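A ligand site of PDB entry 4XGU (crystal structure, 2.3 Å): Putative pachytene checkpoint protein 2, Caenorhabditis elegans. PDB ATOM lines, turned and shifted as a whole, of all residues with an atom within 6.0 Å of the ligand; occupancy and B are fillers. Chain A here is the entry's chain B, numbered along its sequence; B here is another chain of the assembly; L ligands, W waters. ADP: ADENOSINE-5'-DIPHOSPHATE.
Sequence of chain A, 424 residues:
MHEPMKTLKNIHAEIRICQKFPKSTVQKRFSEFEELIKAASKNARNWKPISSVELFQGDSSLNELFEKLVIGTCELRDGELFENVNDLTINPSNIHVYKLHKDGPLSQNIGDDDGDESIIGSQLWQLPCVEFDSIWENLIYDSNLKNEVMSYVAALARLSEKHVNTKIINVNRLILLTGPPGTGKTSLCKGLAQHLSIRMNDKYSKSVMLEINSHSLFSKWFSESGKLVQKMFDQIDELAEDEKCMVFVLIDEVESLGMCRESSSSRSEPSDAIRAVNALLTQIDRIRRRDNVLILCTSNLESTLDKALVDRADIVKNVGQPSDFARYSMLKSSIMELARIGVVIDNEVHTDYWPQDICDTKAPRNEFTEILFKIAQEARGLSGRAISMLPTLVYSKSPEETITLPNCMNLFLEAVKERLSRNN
The backbone carbonyl oxygen of Pro 181 lies close to an oxygen (O1B) of the ligand, 2.5 Å away.
N of Thr 186 is in hydrogen-bond range of O2B of the ligand (2.7 Å).
The side-chain hydroxyl (OG1) of Thr 186 is in hydrogen-bond range of an oxygen (O2B) of the ligand (2.8 Å).
An oxygen (O1A) of the ligand is in hydrogen-bond range of the backbone NH (N) of Ser 187.
OG of Ser 187 lies within hydrogen-bond range of O1A of the ligand (3.2 Å).
N1 of the ligand is in hydrogen-bond range of N of Ile 140 (2.9 Å).
A nitrogen (N6) of the ligand is in hydrogen-bond range of the backbone carbonyl oxygen (O) of Ile 140, 2.8 Å away.
O1B of the ligand sits at hydrogen-bond distance from N of Gly 184 (2.9 Å).
The backbone NH (N) of Lys 185 lies within hydrogen-bond range of an oxygen (O2B) of the ligand (3.0 Å).
The side-chain amino group (NZ) of Lys 185 is in salt-bridge range of an oxygen (O1B) of the ligand (3.1 Å).
OH of Tyr 141 sits at hydrogen-bond distance from O of Gly 184 (3.5 Å).
OD1 of Asn 300 lies within hydrogen-bond range of NZ of Lys 185 (2.5 Å).
NZ of Lys 185 sits close to OG1 of Thr 298, at 3.5 Å.
The side-chain hydroxyl of Tyr 141 is in hydrogen-bond range of the backbone carbonyl oxygen of Thr 183, 2.7 Å away.
The side-chain hydroxyl (OG1) of Thr 183 lies within hydrogen-bond range of the backbone carbonyl oxygen (O) of Pro 180.
The backbone NH (N) of Arg 385 sits at hydrogen-bond distance from the backbone carbonyl oxygen (O) of Gly 182, at 3.2 Å.
The backbone carbonyl oxygen (O) of Gly 182 lies within hydrogen-bond range of the backbone NH (N) of Gly 384.
The side-chain hydroxyl of Ser 388 is in hydrogen-bond range of the backbone carbonyl oxygen of Gly 384, 3.3 Å away.
A nitrogen (N7) of the ligand lies close to the backbone carbonyl oxygen (O) of Thr 183 (3.0 Å).
Merely in contact with the ligand: Asn 138 (3.2 Å), Arg 385 (3.2 Å), Gly 182 (3.3 Å), Met 330 (3.4 Å), Ser 388 (3.5 Å), Tyr 141 (3.6 Å), Asn 300 (3.6 Å), Leu 139 (3.7 Å), Gly 384 (3.8 Å), Pro 180 (3.8 Å) and Lys 167 of chain B (3.97 Å).
Hydrophobic or aromatic side chains that line the ligand: Ile 140, Tyr 141 and Met 330.
18 residues have an atom within 4 Å of the ligand: Asn 138, Leu 139, Ile 140, Tyr 141, Pro 180, Pro 181, Gly 182, Thr 183, Gly 184, Lys 185, Thr 186, Ser 187, Asn 300, Met 330, Gly 384, Arg 385, Ser 388 and Lys 167 of chain B.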
ATOM      1  N   ASN A 138     -12.047  29.378  -6.850  1.00  0.00           N
ATOM      2  CA  ASN A 138     -11.956  28.127  -6.118  1.00  0.00           C
ATOM      3  C   ASN A 138     -12.018  28.319  -4.608  1.00  0.00           C
ATOM      4  O   ASN A 138     -12.062  27.351  -3.852  1.00  0.00           O
ATOM      5  CB  ASN A 138     -10.669  27.394  -6.497  1.00  0.00           C
ATOM      6  CG  ASN A 138     -10.584  27.135  -7.979  1.00  0.00           C
ATOM      7  OD1 ASN A 138     -11.525  26.609  -8.571  1.00  0.00           O
ATOM      8  ND2 ASN A 138      -9.466  27.510  -8.591  1.00  0.00           N
ATOM      9  N   LEU A 139     -12.035  29.576  -4.174  1.00  0.00           N
ATOM     10  CA  LEU A 139     -12.241  29.888  -2.766  1.00  0.00           C
ATOM     11  C   LEU A 139     -13.707  29.747  -2.415  1.00  0.00           C
ATOM     12  O   LEU A 139     -14.568  30.360  -3.057  1.00  0.00           O
ATOM     13  CB  LEU A 139     -11.732  31.295  -2.446  1.00  0.00           C
ATOM     14  CG  LEU A 139     -10.206  31.445  -2.411  1.00  0.00           C
ATOM     15  CD1 LEU A 139      -9.798  32.888  -2.192  1.00  0.00           C
ATOM     16  CD2 LEU A 139      -9.617  30.560  -1.338  1.00  0.00           C
ATOM     17  N   ILE A 140     -14.007  28.928  -1.409  1.00  0.00           N
ATOM     18  CA  ILE A 140     -15.389  28.603  -1.056  1.00  0.00           C
ATOM     19  C   ILE A 140     -15.777  29.034   0.354  1.00  0.00           C
ATOM     20  O   ILE A 140     -15.211  28.564   1.341  1.00  0.00           O
ATOM     21  CB  ILE A 140     -15.639  27.092  -1.164  1.00  0.00           C
ATOM     22  CG1 ILE A 140     -15.257  26.592  -2.558  1.00  0.00           C
ATOM     23  CG2 ILE A 140     -17.100  26.783  -0.859  1.00  0.00           C
ATOM     24  CD1 ILE A 140     -15.482  25.102  -2.747  1.00  0.00           C
ATOM     25  N   TYR A 141     -16.767  29.917   0.435  1.00  0.00           N
ATOM     26  CA  TYR A 141     -17.283  30.370   1.719  1.00  0.00           C
ATOM     27  C   TYR A 141     -18.805  30.383   1.695  1.00  0.00           C
ATOM     28  O   TYR A 141     -19.416  30.452   0.631  1.00  0.00           O
ATOM     29  CB  TYR A 141     -16.738  31.754   2.068  1.00  0.00           C
ATOM     30  CG  TYR A 141     -15.232  31.788   2.273  1.00  0.00           C
ATOM     31  CD1 TYR A 141     -14.663  31.310   3.445  1.00  0.00           C
ATOM     32  CD2 TYR A 141     -14.396  32.299   1.298  1.00  0.00           C
ATOM     33  CE1 TYR A 141     -13.294  31.336   3.635  1.00  0.00           C
ATOM     34  CE2 TYR A 141     -13.024  32.337   1.479  1.00  0.00           C
ATOM     35  CZ  TYR A 141     -12.478  31.850   2.646  1.00  0.00           C
ATOM     36  OH  TYR A 141     -11.122  31.879   2.835  1.00  0.00           O
ATOM     37  N   PRO A 180      -8.330  30.976  12.089  1.00  0.00           N
ATOM     38  CA  PRO A 180      -7.467  29.786  12.128  1.00  0.00           C
ATOM     39  C   PRO A 180      -6.622  29.671  10.857  1.00  0.00           C
ATOM     40  O   PRO A 180      -6.994  30.246   9.830  1.00  0.00           O
ATOM     41  CB  PRO A 180      -8.461  28.637  12.237  1.00  0.00           C
ATOM     42  CG  PRO A 180      -9.675  29.246  12.852  1.00  0.00           C
ATOM     43  CD  PRO A 180      -9.745  30.631  12.293  1.00  0.00           C
ATOM     44  N   PRO A 181      -5.495  28.953  10.920  1.00  0.00           N
ATOM     45  CA  PRO A 181      -4.560  28.811   9.794  1.00  0.00           C
ATOM     46  C   PRO A 181      -5.157  28.136   8.554  1.00  0.00           C
ATOM     47  O   PRO A 181      -4.658  28.364   7.447  1.00  0.00           O
ATOM     48  CB  PRO A 181      -3.440  27.945  10.370  1.00  0.00           C
ATOM     49  CG  PRO A 181      -3.511  28.143  11.838  1.00  0.00           C
ATOM     50  CD  PRO A 181      -4.973  28.303  12.141  1.00  0.00           C
ATOM     51  N   GLY A 182      -6.193  27.325   8.716  1.00  0.00           N
ATOM     52  CA  GLY A 182      -6.696  26.545   7.593  1.00  0.00           C
ATOM     53  C   GLY A 182      -7.768  27.208   6.754  1.00  0.00           C
ATOM     54  O   GLY A 182      -8.304  26.597   5.831  1.00  0.00           O
ATOM     55  N   THR A 183      -8.067  28.471   7.055  1.00  0.00           N
ATOM     56  CA  THR A 183      -9.207  29.152   6.435  1.00  0.00           C
ATOM     57  C   THR A 183      -8.884  29.784   5.079  1.00  0.00           C
ATOM     58  O   THR A 183      -9.788  30.112   4.308  1.00  0.00           O
ATOM     59  CB  THR A 183      -9.734  30.251   7.361  1.00  0.00           C
ATOM     60  OG1 THR A 183      -8.747  31.279   7.501  1.00  0.00           O
ATOM     61  CG2 THR A 183     -10.061  29.678   8.721  1.00  0.00           C
ATOM     62  N   GLY A 184      -7.598  29.954   4.789  1.00  0.00           N
ATOM     63  CA  GLY A 184      -7.183  30.486   3.496  1.00  0.00           C
ATOM     64  C   GLY A 184      -7.238  31.991   3.378  1.00  0.00           C
ATOM     65  O   GLY A 184      -7.720  32.522   2.378  1.00  0.00           O
ATOM     66  N   LYS A 185      -6.747  32.679   4.395  1.00  0.00           N
ATOM     67  CA  LYS A 185      -6.721  34.136   4.402  1.00  0.00           C
ATOM     68  C   LYS A 185      -5.744  34.678   3.370  1.00  0.00           C
ATOM     69  O   LYS A 185      -5.999  35.687   2.723  1.00  0.00           O
ATOM     70  CB  LYS A 185      -6.351  34.653   5.790  1.00  0.00           C
ATOM     71  CG  LYS A 185      -7.150  34.008   6.908  1.00  0.00           C
ATOM     72  CD  LYS A 185      -6.714  34.552   8.258  1.00  0.00           C
ATOM     73  CE  LYS A 185      -6.250  33.427   9.156  1.00  0.00           C
ATOM     74  NZ  LYS A 185      -5.051  32.725   8.616  1.00  0.00           N
ATOM     75  N   THR A 186      -4.607  34.001   3.234  1.00  0.00           N
ATOM     76  CA  THR A 186      -3.589  34.399   2.265  1.00  0.00           C
ATOM     77  C   THR A 186      -4.149  34.331   0.861  1.00  0.00           C
ATOM     78  O   THR A 186      -3.965  35.256   0.070  1.00  0.00           O
ATOM     79  CB  THR A 186      -2.343  33.510   2.368  1.00  0.00           C
ATOM     80  OG1 THR A 186      -1.827  33.536   3.705  1.00  0.00           O
ATOM     81  CG2 THR A 186      -1.268  33.993   1.406  1.00  0.00           C
ATOM     82  N   SER A 187      -4.837  33.230   0.549  1.00  0.00           N
ATOM     83  CA  SER A 187      -5.440  33.039  -0.768  1.00  0.00           C
ATOM     84  C   SER A 187      -6.419  34.152  -1.099  1.00  0.00           C
ATOM     85  O   SER A 187      -6.499  34.600  -2.242  1.00  0.00           O
ATOM     86  CB  SER A 187      -6.128  31.675  -0.846  1.00  0.00           C
ATOM     87  OG  SER A 187      -5.186  30.618  -0.801  1.00  0.00           O
ATOM     88  N   LEU A 188      -7.172  34.590  -0.088  1.00  0.00           N
ATOM     89  CA  LEU A 188      -8.076  35.722  -0.258  1.00  0.00           C
ATOM     90  C   LEU A 188      -7.310  36.978  -0.671  1.00  0.00           C
ATOM     91  O   LEU A 188      -7.714  37.674  -1.602  1.00  0.00           O
ATOM     92  CB  LEU A 188      -8.846  35.996   1.038  1.00  0.00           C
ATOM     93  CG  LEU A 188     -10.041  35.097   1.365  1.00  0.00           C
ATOM     94  CD1 LEU A 188     -10.662  35.505   2.688  1.00  0.00           C
ATOM     95  CD2 LEU A 188     -11.065  35.164   0.244  1.00  0.00           C
ATOM     96  N   THR A 298      -2.577  39.261   7.422  1.00  0.00           N
ATOM     97  CA  THR A 298      -3.291  38.074   7.867  1.00  0.00           C
ATOM     98  C   THR A 298      -2.722  37.592   9.196  1.00  0.00           C
ATOM     99  O   THR A 298      -1.503  37.580   9.385  1.00  0.00           O
ATOM    100  CB  THR A 298      -3.234  36.938   6.825  1.00  0.00           C
ATOM    101  OG1 THR A 298      -3.722  35.720   7.414  1.00  0.00           O
ATOM    102  CG2 THR A 298      -1.818  36.712   6.346  1.00  0.00           C
ATOM    103  N   ASN A 300      -2.834  34.329  11.798  1.00  0.00           N
ATOM    104  CA  ASN A 300      -3.254  32.950  11.976  1.00  0.00           C
ATOM    105  C   ASN A 300      -3.774  32.676  13.388  1.00  0.00           C
ATOM    106  O   ASN A 300      -4.426  31.663  13.631  1.00  0.00           O
ATOM    107  CB  ASN A 300      -2.095  31.996  11.650  1.00  0.00           C
ATOM    108  CG  ASN A 300      -1.817  31.902  10.168  1.00  0.00           C
ATOM    109  OD1 ASN A 300      -2.723  32.063   9.338  1.00  0.00           O
ATOM    110  ND2 ASN A 300      -0.569  31.635   9.805  1.00  0.00           N
ATOM    111  N   PRO A 322     -14.562  26.270   7.713  1.00  0.00           N
ATOM    112  CA  PRO A 322     -15.759  26.105   6.885  1.00  0.00           C
ATOM    113  C   PRO A 322     -16.884  25.373   7.613  1.00  0.00           C
ATOM    114  O   PRO A 322     -16.627  24.448   8.387  1.00  0.00           O
ATOM    115  CB  PRO A 322     -15.252  25.267   5.703  1.00  0.00           C
ATOM    116  CG  PRO A 322     -14.033  24.573   6.215  1.00  0.00           C
ATOM    117  CD  PRO A 322     -13.400  25.556   7.159  1.00  0.00           C
ATOM    118  N   MET A 330     -16.521  21.905  -0.835  1.00  0.00           N
ATOM    119  CA  MET A 330     -15.132  21.588  -1.101  1.00  0.00           C
ATOM    120  C   MET A 330     -14.967  20.136  -1.540  1.00  0.00           C
ATOM    121  O   MET A 330     -14.258  19.848  -2.503  1.00  0.00           O
ATOM    122  CB  MET A 330     -14.278  21.856   0.132  1.00  0.00           C
ATOM    123  CG  MET A 330     -14.322  23.284   0.624  1.00  0.00           C
ATOM    124  SD  MET A 330     -13.349  23.504   2.120  1.00  0.00           S
ATOM    125  CE  MET A 330     -13.600  25.241   2.452  1.00  0.00           C
ATOM    126  N   GLY A 384      -9.945  23.939   6.166  1.00  0.00           N
ATOM    127  CA  GLY A 384     -10.074  24.106   4.725  1.00  0.00           C
ATOM    128  C   GLY A 384      -8.894  23.526   3.987  1.00  0.00           C
ATOM    129  O   GLY A 384      -9.057  22.857   2.966  1.00  0.00           O
ATOM    130  N   ARG A 385      -7.692  23.768   4.511  1.00  0.00           N
ATOM    131  CA  ARG A 385      -6.483  23.225   3.908  1.00  0.00           C
ATOM    132  C   ARG A 385      -6.490  21.711   3.984  1.00  0.00           C
ATOM    133  O   ARG A 385      -6.141  21.040   3.022  1.00  0.00           O
ATOM    134  CB  ARG A 385      -5.228  23.783   4.589  1.00  0.00           C
ATOM    135  CG  ARG A 385      -3.931  23.380   3.910  1.00  0.00           C
ATOM    136  CD  ARG A 385      -2.721  23.954   4.644  1.00  0.00           C
ATOM    137  NE  ARG A 385      -1.488  23.769   3.885  1.00  0.00           N
ATOM    138  CZ  ARG A 385      -0.694  22.710   3.975  1.00  0.00           C
ATOM    139  NH1 ARG A 385      -0.993  21.725   4.819  1.00  0.00           N
ATOM    140  NH2 ARG A 385       0.410  22.630   3.240  1.00  0.00           N
ATOM    141  N   ALA A 386      -6.899  21.183   5.135  1.00  0.00           N
ATOM    142  CA  ALA A 386      -6.938  19.740   5.360  1.00  0.00           C
ATOM    143  C   ALA A 386      -7.893  19.045   4.380  1.00  0.00           C
ATOM    144  O   ALA A 386      -7.620  17.938   3.931  1.00  0.00           O
ATOM    145  CB  ALA A 386      -7.349  19.437   6.791  1.00  0.00           C
ATOM    146  N   SER A 388      -8.524  20.105   1.396  1.00  0.00           N
ATOM    147  CA  SER A 388      -7.805  20.141   0.126  1.00  0.00           C
ATOM    148  C   SER A 388      -6.759  19.037   0.051  1.00  0.00           C
ATOM    149  O   SER A 388      -6.391  18.585  -1.023  1.00  0.00           O
ATOM    150  CB  SER A 388      -7.148  21.501  -0.085  1.00  0.00           C
ATOM    151  OG  SER A 388      -8.112  22.523  -0.191  1.00  0.00           O
ATOM    152  N   THR B 166      -4.179  22.965  -8.744  1.00  0.00           N
ATOM    153  CA  THR B 166      -3.658  23.114  -7.390  1.00  0.00           C
ATOM    154  C   THR B 166      -4.667  23.785  -6.464  1.00  0.00           C
ATOM    155  O   THR B 166      -4.785  23.419  -5.288  1.00  0.00           O
ATOM    156  CB  THR B 166      -2.334  23.931  -7.390  1.00  0.00           C
ATOM    157  OG1 THR B 166      -1.336  23.218  -8.117  1.00  0.00           O
ATOM    158  CG2 THR B 166      -1.844  24.187  -5.980  1.00  0.00           C
ATOM    159  N   LYS B 167      -5.409  24.749  -6.979  1.00  0.00           N
ATOM    160  CA  LYS B 167      -6.284  25.568  -6.150  1.00  0.00           C
ATOM    161  C   LYS B 167      -7.548  24.840  -5.700  1.00  0.00           C
ATOM    162  O   LYS B 167      -8.183  25.233  -4.722  1.00  0.00           O
ATOM    163  CB  LYS B 167      -6.671  26.859  -6.876  1.00  0.00           C
ATOM    164  CG  LYS B 167      -5.543  27.868  -6.981  1.00  0.00           C
ATOM    165  CD  LYS B 167      -4.607  27.550  -8.121  1.00  0.00           C
ATOM    166  CE  LYS B 167      -3.427  28.513  -8.166  1.00  0.00           C
ATOM    167  NZ  LYS B 167      -2.527  28.336  -6.991  1.00  0.00           N
ATOM    168  N   ILE B 168      -7.918  23.782  -6.417  1.00  0.00           N
ATOM    169  CA  ILE B 168      -9.043  22.958  -6.011  1.00  0.00           C
ATOM    170  C   ILE B 168      -8.534  21.843  -5.110  1.00  0.00           C
ATOM    171  O   ILE B 168      -9.018  21.666  -3.993  1.00  0.00           O
ATOM    172  CB  ILE B 168      -9.796  22.358  -7.215  1.00  0.00           C
ATOM    173  CG1 ILE B 168     -10.366  23.467  -8.095  1.00  0.00           C
ATOM    174  CG2 ILE B 168     -10.901  21.433  -6.743  1.00  0.00           C
ATOM    175  CD1 ILE B 168     -10.903  22.976  -9.420  1.00  0.00           C
ATOM    176  N   ASN B 170      -5.119  20.637  -3.326  1.00  0.00           N
ATOM    177  CA  ASN B 170      -3.790  21.113  -2.979  1.00  0.00           C
ATOM    178  C   ASN B 170      -2.746  20.010  -3.030  1.00  0.00           C
ATOM    179  O   ASN B 170      -2.780  19.058  -2.261  1.00  0.00           O
ATOM    180  CB  ASN B 170      -3.795  21.753  -1.584  1.00  0.00           C
ATOM    181  CG  ASN B 170      -2.557  22.586  -1.325  1.00  0.00           C
ATOM    182  OD1 ASN B 170      -1.917  23.062  -2.265  1.00  0.00           O
ATOM    183  ND2 ASN B 170      -2.225  22.769  -0.054  1.00  0.00           N
HETATM  184  PB  ADP L   1      -4.043  30.692   5.590  1.00  0.00           P
HETATM  185  O1B ADP L   1      -5.322  30.583   6.393  1.00  0.00           O
HETATM  186  O2B ADP L   1      -3.839  32.038   4.949  1.00  0.00           O
HETATM  187  O3B ADP L   1      -2.823  30.149   6.301  1.00  0.00           O
HETATM  188  PA  ADP L   1      -3.665  29.934   2.895  1.00  0.00           P
HETATM  189  O1A ADP L   1      -4.377  31.110   2.286  1.00  0.00           O
HETATM  190  O2A ADP L   1      -2.156  29.939   3.019  1.00  0.00           O
HETATM  191  O3A ADP L   1      -4.288  29.675   4.363  1.00  0.00           O
HETATM  192  O5' ADP L   1      -4.070  28.635   2.039  1.00  0.00           O
HETATM  193  C5' ADP L   1      -4.689  27.499   2.645  1.00  0.00           C
HETATM  194  C4' ADP L   1      -4.913  26.433   1.571  1.00  0.00           C
HETATM  195  O4' ADP L   1      -6.060  25.655   1.902  1.00  0.00           O
HETATM  196  C3' ADP L   1      -5.165  27.070   0.208  1.00  0.00           C
HETATM  197  O3' ADP L   1      -4.053  26.835  -0.660  1.00  0.00           O
HETATM  198  C2' ADP L   1      -6.408  26.406  -0.325  1.00  0.00           C
HETATM  199  O2' ADP L   1      -6.064  25.485  -1.370  1.00  0.00           O
HETATM  200  C1' ADP L   1      -7.016  25.643   0.841  1.00  0.00           C
HETATM  201  N9  ADP L   1      -8.225  26.379   1.316  1.00  0.00           N
HETATM  202  C8  ADP L   1      -8.340  26.987   2.512  1.00  0.00           C
HETATM  203  N7  ADP L   1      -9.550  27.577   2.655  1.00  0.00           N
HETATM  204  C5  ADP L   1     -10.244  27.334   1.536  1.00  0.00           C
HETATM  205  C6  ADP L   1     -11.595  27.675   1.028  1.00  0.00           C
HETATM  206  N6  ADP L   1     -12.451  28.400   1.791  1.00  0.00           N
HETATM  207  N1  ADP L   1     -11.937  27.244  -0.199  1.00  0.00           N
HETATM  208  C2  ADP L   1     -11.081  26.525  -0.954  1.00  0.00           C
HETATM  209  N3  ADP L   1      -9.835  26.184  -0.569  1.00  0.00           N
HETATM  210  C4  ADP L   1      -9.366  26.552   0.651  1.00  0.00           C
HETATM  211  O   HOH W   1      -0.624  27.077  -0.954  1.00  0.00           O
